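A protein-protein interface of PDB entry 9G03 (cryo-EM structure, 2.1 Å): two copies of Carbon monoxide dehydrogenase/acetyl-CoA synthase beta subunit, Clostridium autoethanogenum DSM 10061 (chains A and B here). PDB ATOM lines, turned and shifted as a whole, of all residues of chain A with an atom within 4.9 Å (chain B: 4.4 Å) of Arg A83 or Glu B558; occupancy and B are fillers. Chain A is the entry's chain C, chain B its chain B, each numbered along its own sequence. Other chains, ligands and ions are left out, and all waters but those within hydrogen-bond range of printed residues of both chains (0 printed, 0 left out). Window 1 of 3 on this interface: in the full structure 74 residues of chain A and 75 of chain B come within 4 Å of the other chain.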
ATOM      1  N   ASN A  48       7.766 -30.566  15.003  1.00  0.00           N
ATOM      2  CA  ASN A  48       7.039 -30.563  16.264  1.00  0.00           C
ATOM      3  C   ASN A  48       7.662 -31.459  17.334  1.00  0.00           C
ATOM      4  O   ASN A  48       7.288 -31.326  18.499  1.00  0.00           O
ATOM      5  CB  ASN A  48       5.579 -30.950  16.010  1.00  0.00           C
ATOM      6  CG  ASN A  48       4.802 -29.836  15.311  1.00  0.00           C
ATOM      7  OD1 ASN A  48       5.398 -28.914  14.772  1.00  0.00           O
ATOM      8  ND2 ASN A  48       3.476 -29.924  15.314  1.00  0.00           N
ATOM      9  N   ARG A  79      -1.562 -29.280  10.958  1.00  0.00           N
ATOM     10  CA  ARG A  79      -0.999 -28.826  12.227  1.00  0.00           C
ATOM     11  C   ARG A  79      -0.259 -27.502  12.063  1.00  0.00           C
ATOM     12  O   ARG A  79      -0.426 -26.594  12.884  1.00  0.00           O
ATOM     13  CB  ARG A  79      -0.089 -29.904  12.826  1.00  0.00           C
ATOM     14  CG  ARG A  79      -0.842 -31.170  13.241  1.00  0.00           C
ATOM     15  CD  ARG A  79       0.014 -32.132  14.060  1.00  0.00           C
ATOM     16  NE  ARG A  79       1.236 -32.536  13.373  1.00  0.00           N
ATOM     17  CZ  ARG A  79       2.009 -33.541  13.760  1.00  0.00           C
ATOM     18  NH1 ARG A  79       1.688 -34.295  14.797  1.00  0.00           N
ATOM     19  NH2 ARG A  79       3.134 -33.793  13.095  1.00  0.00           N
ATOM     20  N   ASN A  80       0.521 -27.352  10.988  1.00  0.00           N
ATOM     21  CA  ASN A  80       1.203 -26.080  10.750  1.00  0.00           C
ATOM     22  C   ASN A  80       0.201 -24.931  10.597  1.00  0.00           C
ATOM     23  O   ASN A  80       0.376 -23.855  11.187  1.00  0.00           O
ATOM     24  CB  ASN A  80       2.080 -26.191   9.498  1.00  0.00           C
ATOM     25  CG  ASN A  80       3.285 -27.102   9.698  1.00  0.00           C
ATOM     26  OD1 ASN A  80       3.723 -27.331  10.818  1.00  0.00           O
ATOM     27  ND2 ASN A  80       3.819 -27.620   8.607  1.00  0.00           N
ATOM     28  N   PHE A  81      -0.869 -25.153   9.832  1.00  0.00           N
ATOM     29  CA  PHE A  81      -1.895 -24.124   9.663  1.00  0.00           C
ATOM     30  C   PHE A  81      -2.551 -23.773  10.995  1.00  0.00           C
ATOM     31  O   PHE A  81      -2.719 -22.591  11.323  1.00  0.00           O
ATOM     32  CB  PHE A  81      -2.947 -24.596   8.658  1.00  0.00           C
ATOM     33  CG  PHE A  81      -4.028 -23.583   8.384  1.00  0.00           C
ATOM     34  CD1 PHE A  81      -3.875 -22.655   7.371  1.00  0.00           C
ATOM     35  CD2 PHE A  81      -5.207 -23.568   9.122  1.00  0.00           C
ATOM     36  CE1 PHE A  81      -4.858 -21.723   7.106  1.00  0.00           C
ATOM     37  CE2 PHE A  81      -6.199 -22.628   8.853  1.00  0.00           C
ATOM     38  CZ  PHE A  81      -6.013 -21.709   7.845  1.00  0.00           C
ATOM     39  N   ALA A  82      -2.872 -24.788  11.800  1.00  0.00           N
ATOM     40  CA  ALA A  82      -3.502 -24.551  13.094  1.00  0.00           C
ATOM     41  C   ALA A  82      -2.597 -23.736  14.005  1.00  0.00           C
ATOM     42  O   ALA A  82      -3.068 -22.842  14.711  1.00  0.00           O
ATOM     43  CB  ALA A  82      -3.860 -25.883  13.755  1.00  0.00           C
ATOM     44  N   ARG A  83      -1.294 -24.006  13.975  1.00  0.00           N
ATOM     45  CA  ARG A  83      -0.368 -23.245  14.810  1.00  0.00           C
ATOM     46  C   ARG A  83      -0.256 -21.800  14.328  1.00  0.00           C
ATOM     47  O   ARG A  83      -0.128 -20.883  15.148  1.00  0.00           O
ATOM     48  CB  ARG A  83       1.004 -23.929  14.861  1.00  0.00           C
ATOM     49  CG  ARG A  83       1.009 -25.209  15.712  1.00  0.00           C
ATOM     50  CD  ARG A  83       2.365 -25.540  16.342  1.00  0.00           C
ATOM     51  NE  ARG A  83       2.242 -26.646  17.284  1.00  0.00           N
ATOM     52  CZ  ARG A  83       3.247 -27.255  17.901  1.00  0.00           C
ATOM     53  NH1 ARG A  83       4.504 -26.910  17.688  1.00  0.00           N
ATOM     54  NH2 ARG A  83       2.977 -28.234  18.759  1.00  0.00           N
ATOM     55  N   MET A  84      -0.321 -21.568  13.016  1.00  0.00           N
ATOM     56  CA  MET A  84      -0.366 -20.181  12.548  1.00  0.00           C
ATOM     57  C   MET A  84      -1.604 -19.467  13.090  1.00  0.00           C
ATOM     58  O   MET A  84      -1.523 -18.318  13.553  1.00  0.00           O
ATOM     59  CB  MET A  84      -0.366 -20.127  11.023  1.00  0.00           C
ATOM     60  CG  MET A  84       0.860 -20.703  10.376  1.00  0.00           C
ATOM     61  SD  MET A  84       0.852 -20.430   8.596  1.00  0.00           S
ATOM     62  CE  MET A  84       1.294 -18.703   8.527  1.00  0.00           C
ATOM     63  N   VAL A  85      -2.757 -20.139  13.039  1.00  0.00           N
ATOM     64  CA  VAL A  85      -3.989 -19.550  13.568  1.00  0.00           C
ATOM     65  C   VAL A  85      -3.850 -19.268  15.066  1.00  0.00           C
ATOM     66  O   VAL A  85      -4.275 -18.215  15.552  1.00  0.00           O
ATOM     67  CB  VAL A  85      -5.194 -20.467  13.277  1.00  0.00           C
ATOM     68  CG1 VAL A  85      -6.411 -20.038  14.090  1.00  0.00           C
ATOM     69  CG2 VAL A  85      -5.538 -20.500  11.768  1.00  0.00           C
ATOM     70  N   ALA A  86      -3.270 -20.208  15.814  1.00  0.00           N
ATOM     71  CA  ALA A  86      -3.114 -20.026  17.254  1.00  0.00           C
ATOM     72  C   ALA A  86      -2.209 -18.840  17.557  1.00  0.00           C
ATOM     73  O   ALA A  86      -2.495 -18.056  18.462  1.00  0.00           O
ATOM     74  CB  ALA A  86      -2.563 -21.293  17.903  1.00  0.00           C
ATOM     75  N   ALA A  87      -1.128 -18.677  16.795  1.00  0.00           N
ATOM     76  CA  ALA A  87      -0.240 -17.538  17.018  1.00  0.00           C
ATOM     77  C   ALA A  87      -0.947 -16.211  16.724  1.00  0.00           C
ATOM     78  O   ALA A  87      -0.835 -15.255  17.504  1.00  0.00           O
ATOM     79  CB  ALA A  87       1.010 -17.678  16.152  1.00  0.00           C
ATOM     80  N   VAL A 189      -5.468 -25.713  20.833  1.00  0.00           N
ATOM     81  CA  VAL A 189      -4.825 -25.879  19.531  1.00  0.00           C
ATOM     82  C   VAL A 189      -3.375 -26.311  19.707  1.00  0.00           C
ATOM     83  O   VAL A 189      -2.916 -27.262  19.066  1.00  0.00           O
ATOM     84  CB  VAL A 189      -4.920 -24.588  18.694  1.00  0.00           C
ATOM     85  CG1 VAL A 189      -3.970 -24.671  17.486  1.00  0.00           C
ATOM     86  CG2 VAL A 189      -6.357 -24.324  18.249  1.00  0.00           C
ATOM     87  N   MET A 190      -2.649 -25.663  20.625  1.00  0.00           N
ATOM     88  CA  MET A 190      -1.260 -26.061  20.848  1.00  0.00           C
ATOM     89  C   MET A 190      -1.150 -27.494  21.363  1.00  0.00           C
ATOM     90  O   MET A 190      -0.196 -28.203  21.024  1.00  0.00           O
ATOM     91  CB  MET A 190      -0.579 -25.097  21.827  1.00  0.00           C
ATOM     92  CG  MET A 190      -0.372 -23.671  21.284  1.00  0.00           C
ATOM     93  SD  MET A 190       0.624 -23.588  19.779  1.00  0.00           S
ATOM     94  CE  MET A 190       2.205 -24.169  20.396  1.00  0.00           C
ATOM     95  N   THR A 193      -1.761 -30.199  18.389  1.00  0.00           N
ATOM     96  CA  THR A 193      -0.684 -30.305  17.412  1.00  0.00           C
ATOM     97  C   THR A 193       0.561 -30.992  17.976  1.00  0.00           C
ATOM     98  O   THR A 193       1.493 -31.263  17.214  1.00  0.00           O
ATOM     99  CB  THR A 193      -0.297 -28.917  16.864  1.00  0.00           C
ATOM    100  OG1 THR A 193       0.068 -28.047  17.938  1.00  0.00           O
ATOM    101  CG2 THR A 193      -1.447 -28.292  16.074  1.00  0.00           C
ATOM    102  N   HIS A 194       0.612 -31.255  19.282  1.00  0.00           N
ATOM    103  CA  HIS A 194       1.736 -31.977  19.869  1.00  0.00           C
ATOM    104  C   HIS A 194       1.880 -33.369  19.247  1.00  0.00           C
ATOM    105  O   HIS A 194       0.899 -33.983  18.825  1.00  0.00           O
ATOM    106  CB  HIS A 194       1.514 -32.099  21.383  1.00  0.00           C
ATOM    107  CG  HIS A 194       2.654 -32.720  22.133  1.00  0.00           C
ATOM    108  ND1 HIS A 194       2.857 -34.081  22.189  1.00  0.00           N
ATOM    109  CD2 HIS A 194       3.628 -32.165  22.891  1.00  0.00           C
ATOM    110  CE1 HIS A 194       3.920 -34.337  22.928  1.00  0.00           C
ATOM    111  NE2 HIS A 194       4.406 -33.192  23.368  1.00  0.00           N
ATOM    112  N   ILE A 195       3.120 -33.867  19.189  1.00  0.00           N
ATOM    113  CA  ILE A 195       3.385 -35.136  18.512  1.00  0.00           C
ATOM    114  C   ILE A 195       2.455 -36.197  19.083  1.00  0.00           C
ATOM    115  O   ILE A 195       2.241 -36.261  20.295  1.00  0.00           O
ATOM    116  CB  ILE A 195       4.874 -35.531  18.624  1.00  0.00           C
ATOM    117  CG1 ILE A 195       5.168 -36.806  17.801  1.00  0.00           C
ATOM    118  CG2 ILE A 195       5.329 -35.661  20.086  1.00  0.00           C
ATOM    119  CD1 ILE A 195       5.033 -38.132  18.564  1.00  0.00           C
ATOM    120  N   GLU A 558       0.820 -14.091  10.858  1.00  0.00           N
ATOM    121  CA  GLU A 558      -0.068 -15.100  11.435  1.00  0.00           C
ATOM    122  C   GLU A 558      -1.401 -14.488  11.848  1.00  0.00           C
ATOM    123  O   GLU A 558      -2.444 -15.141  11.739  1.00  0.00           O
ATOM    124  CB  GLU A 558       0.624 -15.779  12.628  1.00  0.00           C
ATOM    125  CG  GLU A 558       1.776 -16.704  12.228  1.00  0.00           C
ATOM    126  CD  GLU A 558       2.755 -17.010  13.367  1.00  0.00           C
ATOM    127  OE1 GLU A 558       3.133 -16.088  14.117  1.00  0.00           O
ATOM    128  OE2 GLU A 558       3.149 -18.179  13.507  1.00  0.00           O
ATOM    129  N   MET B  84       8.445 -24.556  21.376  1.00  0.00           N
ATOM    130  CA  MET B  84       8.465 -25.931  21.882  1.00  0.00           C
ATOM    131  C   MET B  84       8.032 -25.978  23.345  1.00  0.00           C
ATOM    132  O   MET B  84       7.232 -26.841  23.744  1.00  0.00           O
ATOM    133  CB  MET B  84       9.858 -26.542  21.743  1.00  0.00           C
ATOM    134  CG  MET B  84      10.353 -26.643  20.326  1.00  0.00           C
ATOM    135  SD  MET B  84      11.903 -27.552  20.224  1.00  0.00           S
ATOM    136  CE  MET B  84      11.323 -29.213  20.491  1.00  0.00           C
ATOM    137  N   ALA B  87       4.263 -25.449  23.603  1.00  0.00           N
ATOM    138  CA  ALA B  87       3.504 -26.638  23.223  1.00  0.00           C
ATOM    139  C   ALA B  87       3.522 -27.692  24.333  1.00  0.00           C
ATOM    140  O   ALA B  87       2.481 -28.278  24.664  1.00  0.00           O
ATOM    141  CB  ALA B  87       4.065 -27.218  21.929  1.00  0.00           C
ATOM    142  N   GLY B  88       4.692 -27.946  24.924  1.00  0.00           N
ATOM    143  CA  GLY B  88       4.752 -28.899  26.025  1.00  0.00           C
ATOM    144  C   GLY B  88       3.908 -28.459  27.210  1.00  0.00           C
ATOM    145  O   GLY B  88       3.176 -29.265  27.811  1.00  0.00           O
ATOM    146  N   MET B 190       3.216 -17.405  22.737  1.00  0.00           N
ATOM    147  CA  MET B 190       2.809 -17.418  21.333  1.00  0.00           C
ATOM    148  C   MET B 190       2.754 -16.007  20.751  1.00  0.00           C
ATOM    149  O   MET B 190       3.128 -15.789  19.592  1.00  0.00           O
ATOM    150  CB  MET B 190       1.458 -18.118  21.187  1.00  0.00           C
ATOM    151  CG  MET B 190       1.503 -19.623  21.455  1.00  0.00           C
ATOM    152  SD  MET B 190       2.601 -20.552  20.369  1.00  0.00           S
ATOM    153  CE  MET B 190       1.810 -20.294  18.782  1.00  0.00           C
ATOM    154  N   MET B 556      12.099 -36.928  23.265  1.00  0.00           N
ATOM    155  CA  MET B 556      11.658 -36.561  21.922  1.00  0.00           C
ATOM    156  C   MET B 556      10.603 -35.455  21.896  1.00  0.00           C
ATOM    157  O   MET B 556      10.542 -34.689  20.933  1.00  0.00           O
ATOM    158  CB  MET B 556      11.137 -37.803  21.176  1.00  0.00           C
ATOM    159  CG  MET B 556       9.809 -38.367  21.671  1.00  0.00           C
ATOM    160  SD  MET B 556       8.320 -37.685  20.903  1.00  0.00           S
ATOM    161  CE  MET B 556       7.057 -38.513  21.877  1.00  0.00           C
ATOM    162  N   SER B 557       9.772 -35.355  22.926  1.00  0.00           N
ATOM    163  CA  SER B 557       8.551 -34.564  22.860  1.00  0.00           C
ATOM    164  C   SER B 557       8.793 -33.113  23.290  1.00  0.00           C
ATOM    165  O   SER B 557       9.741 -32.797  24.008  1.00  0.00           O
ATOM    166  CB  SER B 557       7.444 -35.186  23.720  1.00  0.00           C
ATOM    167  OG  SER B 557       7.779 -35.194  25.092  1.00  0.00           O
ATOM    168  N   GLU B 558       7.886 -32.237  22.851  1.00  0.00           N
ATOM    169  CA  GLU B 558       7.871 -30.861  23.345  1.00  0.00           C
ATOM    170  C   GLU B 558       7.598 -30.837  24.846  1.00  0.00           C
ATOM    171  O   GLU B 558       8.143 -29.990  25.563  1.00  0.00           O
ATOM    172  CB  GLU B 558       6.823 -30.040  22.576  1.00  0.00           C
ATOM    173  CG  GLU B 558       7.234 -29.684  21.138  1.00  0.00           C
ATOM    174  CD  GLU B 558       6.070 -29.252  20.235  1.00  0.00           C
ATOM    175  OE1 GLU B 558       4.973 -29.838  20.315  1.00  0.00           O
ATOM    176  OE2 GLU B 558       6.261 -28.321  19.433  1.00  0.00           O
ATOM    177  N   LYS B 559       6.804 -31.789  25.339  1.00  0.00           N
ATOM    178  CA  LYS B 559       6.599 -31.911  26.779  1.00  0.00           C
ATOM    179  C   LYS B 559       7.922 -32.104  27.513  1.00  0.00           C
ATOM    180  O   LYS B 559       8.141 -31.496  28.562  1.00  0.00           O
ATOM    181  CB  LYS B 559       5.676 -33.085  27.084  1.00  0.00           C
ATOM    182  CG  LYS B 559       4.211 -32.793  26.921  1.00  0.00           C
ATOM    183  CD  LYS B 559       3.359 -34.003  27.278  1.00  0.00           C
ATOM    184  CE  LYS B 559       3.549 -35.146  26.273  1.00  0.00           C
ATOM    185  NZ  LYS B 559       2.825 -36.396  26.609  1.00  0.00           N
ATOM    186  N   ALA B 560       8.835 -32.892  26.944  1.00  0.00           N
ATOM    187  CA  ALA B 560      10.146 -33.079  27.561  1.00  0.00           C
ATOM    188  C   ALA B 560      10.918 -31.766  27.627  1.00  0.00           C
ATOM    189  O   ALA B 560      11.598 -31.493  28.622  1.00  0.00           O
ATOM    190  CB  ALA B 560      10.938 -34.138  26.796  1.00  0.00           C
ATOM    191  N   VAL B 561      10.814 -30.936  26.588  1.00  0.00           N
ATOM    192  CA  VAL B 561      11.477 -29.631  26.583  1.00  0.00           C
ATOM    193  C   VAL B 561      10.924 -28.756  27.701  1.00  0.00           C
ATOM    194  O   VAL B 561      11.679 -28.151  28.472  1.00  0.00           O
ATOM    195  CB  VAL B 561      11.324 -28.940  25.215  1.00  0.00           C
ATOM    196  CG1 VAL B 561      11.950 -27.548  25.254  1.00  0.00           C
ATOM    197  CG2 VAL B 561      11.953 -29.769  24.120  1.00  0.00           C
ATOM    198  N   ALA B 562       9.598 -28.696  27.816  1.00  0.00           N
ATOM    199  CA  ALA B 562       8.992 -27.900  28.879  1.00  0.00           C
ATOM    200  C   ALA B 562       9.411 -28.424  30.254  1.00  0.00           C
ATOM    201  O   ALA B 562       9.691 -27.638  31.167  1.00  0.00           O
ATOM    202  CB  ALA B 562       7.470 -27.900  28.726  1.00  0.00           C
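Of the printed residues of chain B, Asn A48 touches Glu B558 (3.0 Å).
Arg A83 touches just these residues of chain B: Ala B87 and Glu B558.
Of the printed residues of chain B, Ile A195 touches Met B556.
Of the printed residues of chain A, Ala B87 touches Arg A83 and Met A190.
Of the printed residues of chain A, Met B556 touches Ile A195.
Of the printed residues of chain A, Ser B557 touches His A194.
Of chain A, only Asn A48 (3.0 Å), Arg A83 (2.9 Å) and His A194 (3.6 Å) come within 4 Å of Glu B558.
The nearest residue of chain B that does not touch Arg A83 is Met B190 (4.2 Å).
Among the printed residues, merely in contact across the chains: Arg A83 with Ala B87 (3.5 Å), Ala A87 with Met B190 (3.8 Å), Met A190 with Ala B87 (3.9 Å), His A194 with Ser B557 (3.7 Å), His A194 with Glu B558 (3.6 Å) and Ile A195 with Met B556 (3.7 Å).
OG of Ser B557 is in hydrogen-bond range of N of Ala B560 (3.1 Å).
ND2 of Asn A48 sits at hydrogen-bond distance from O of Thr A193.
NE of Arg A83 lies within hydrogen-bond range of OG1 of Thr A193, at 2.7 Å.
OG1 of Thr A193 lies within hydrogen-bond range of O of Met A190.
Ala A87 touches Met B190, and with the chains exchanged Met A190 touches Ala B87.
Met B190 touches its own counterpart, Met A190.
Positions printed for both chains: 84, 87, 190 and 558.
Of the 10 pairs that touch across the chains among the printed residues, 3 have their exchanged pair printed and touching as well.
Hydrophobic or aromatic side chains of chain B that line the printed part of chain A: Ala B87, Met B190 and Met B556.
Of the 16 printed residues of chain A, 6 touch a printed residue of chain B.
The guanidinium group (NH1) of Arg A83 lies within salt-bridge range of the side-chain carboxylate (OE2) of Glu B558, at 2.9 Å.
N of Lys B559 lies within hydrogen-bond range of NE2 of His A194.
O of Asn A48 lies close to OE1 of Glu B558 (3.3 Å).
The side-chain sulfur of Met B190 lies close to the side-chain sulfur of Met A190, at 3.7 Å.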
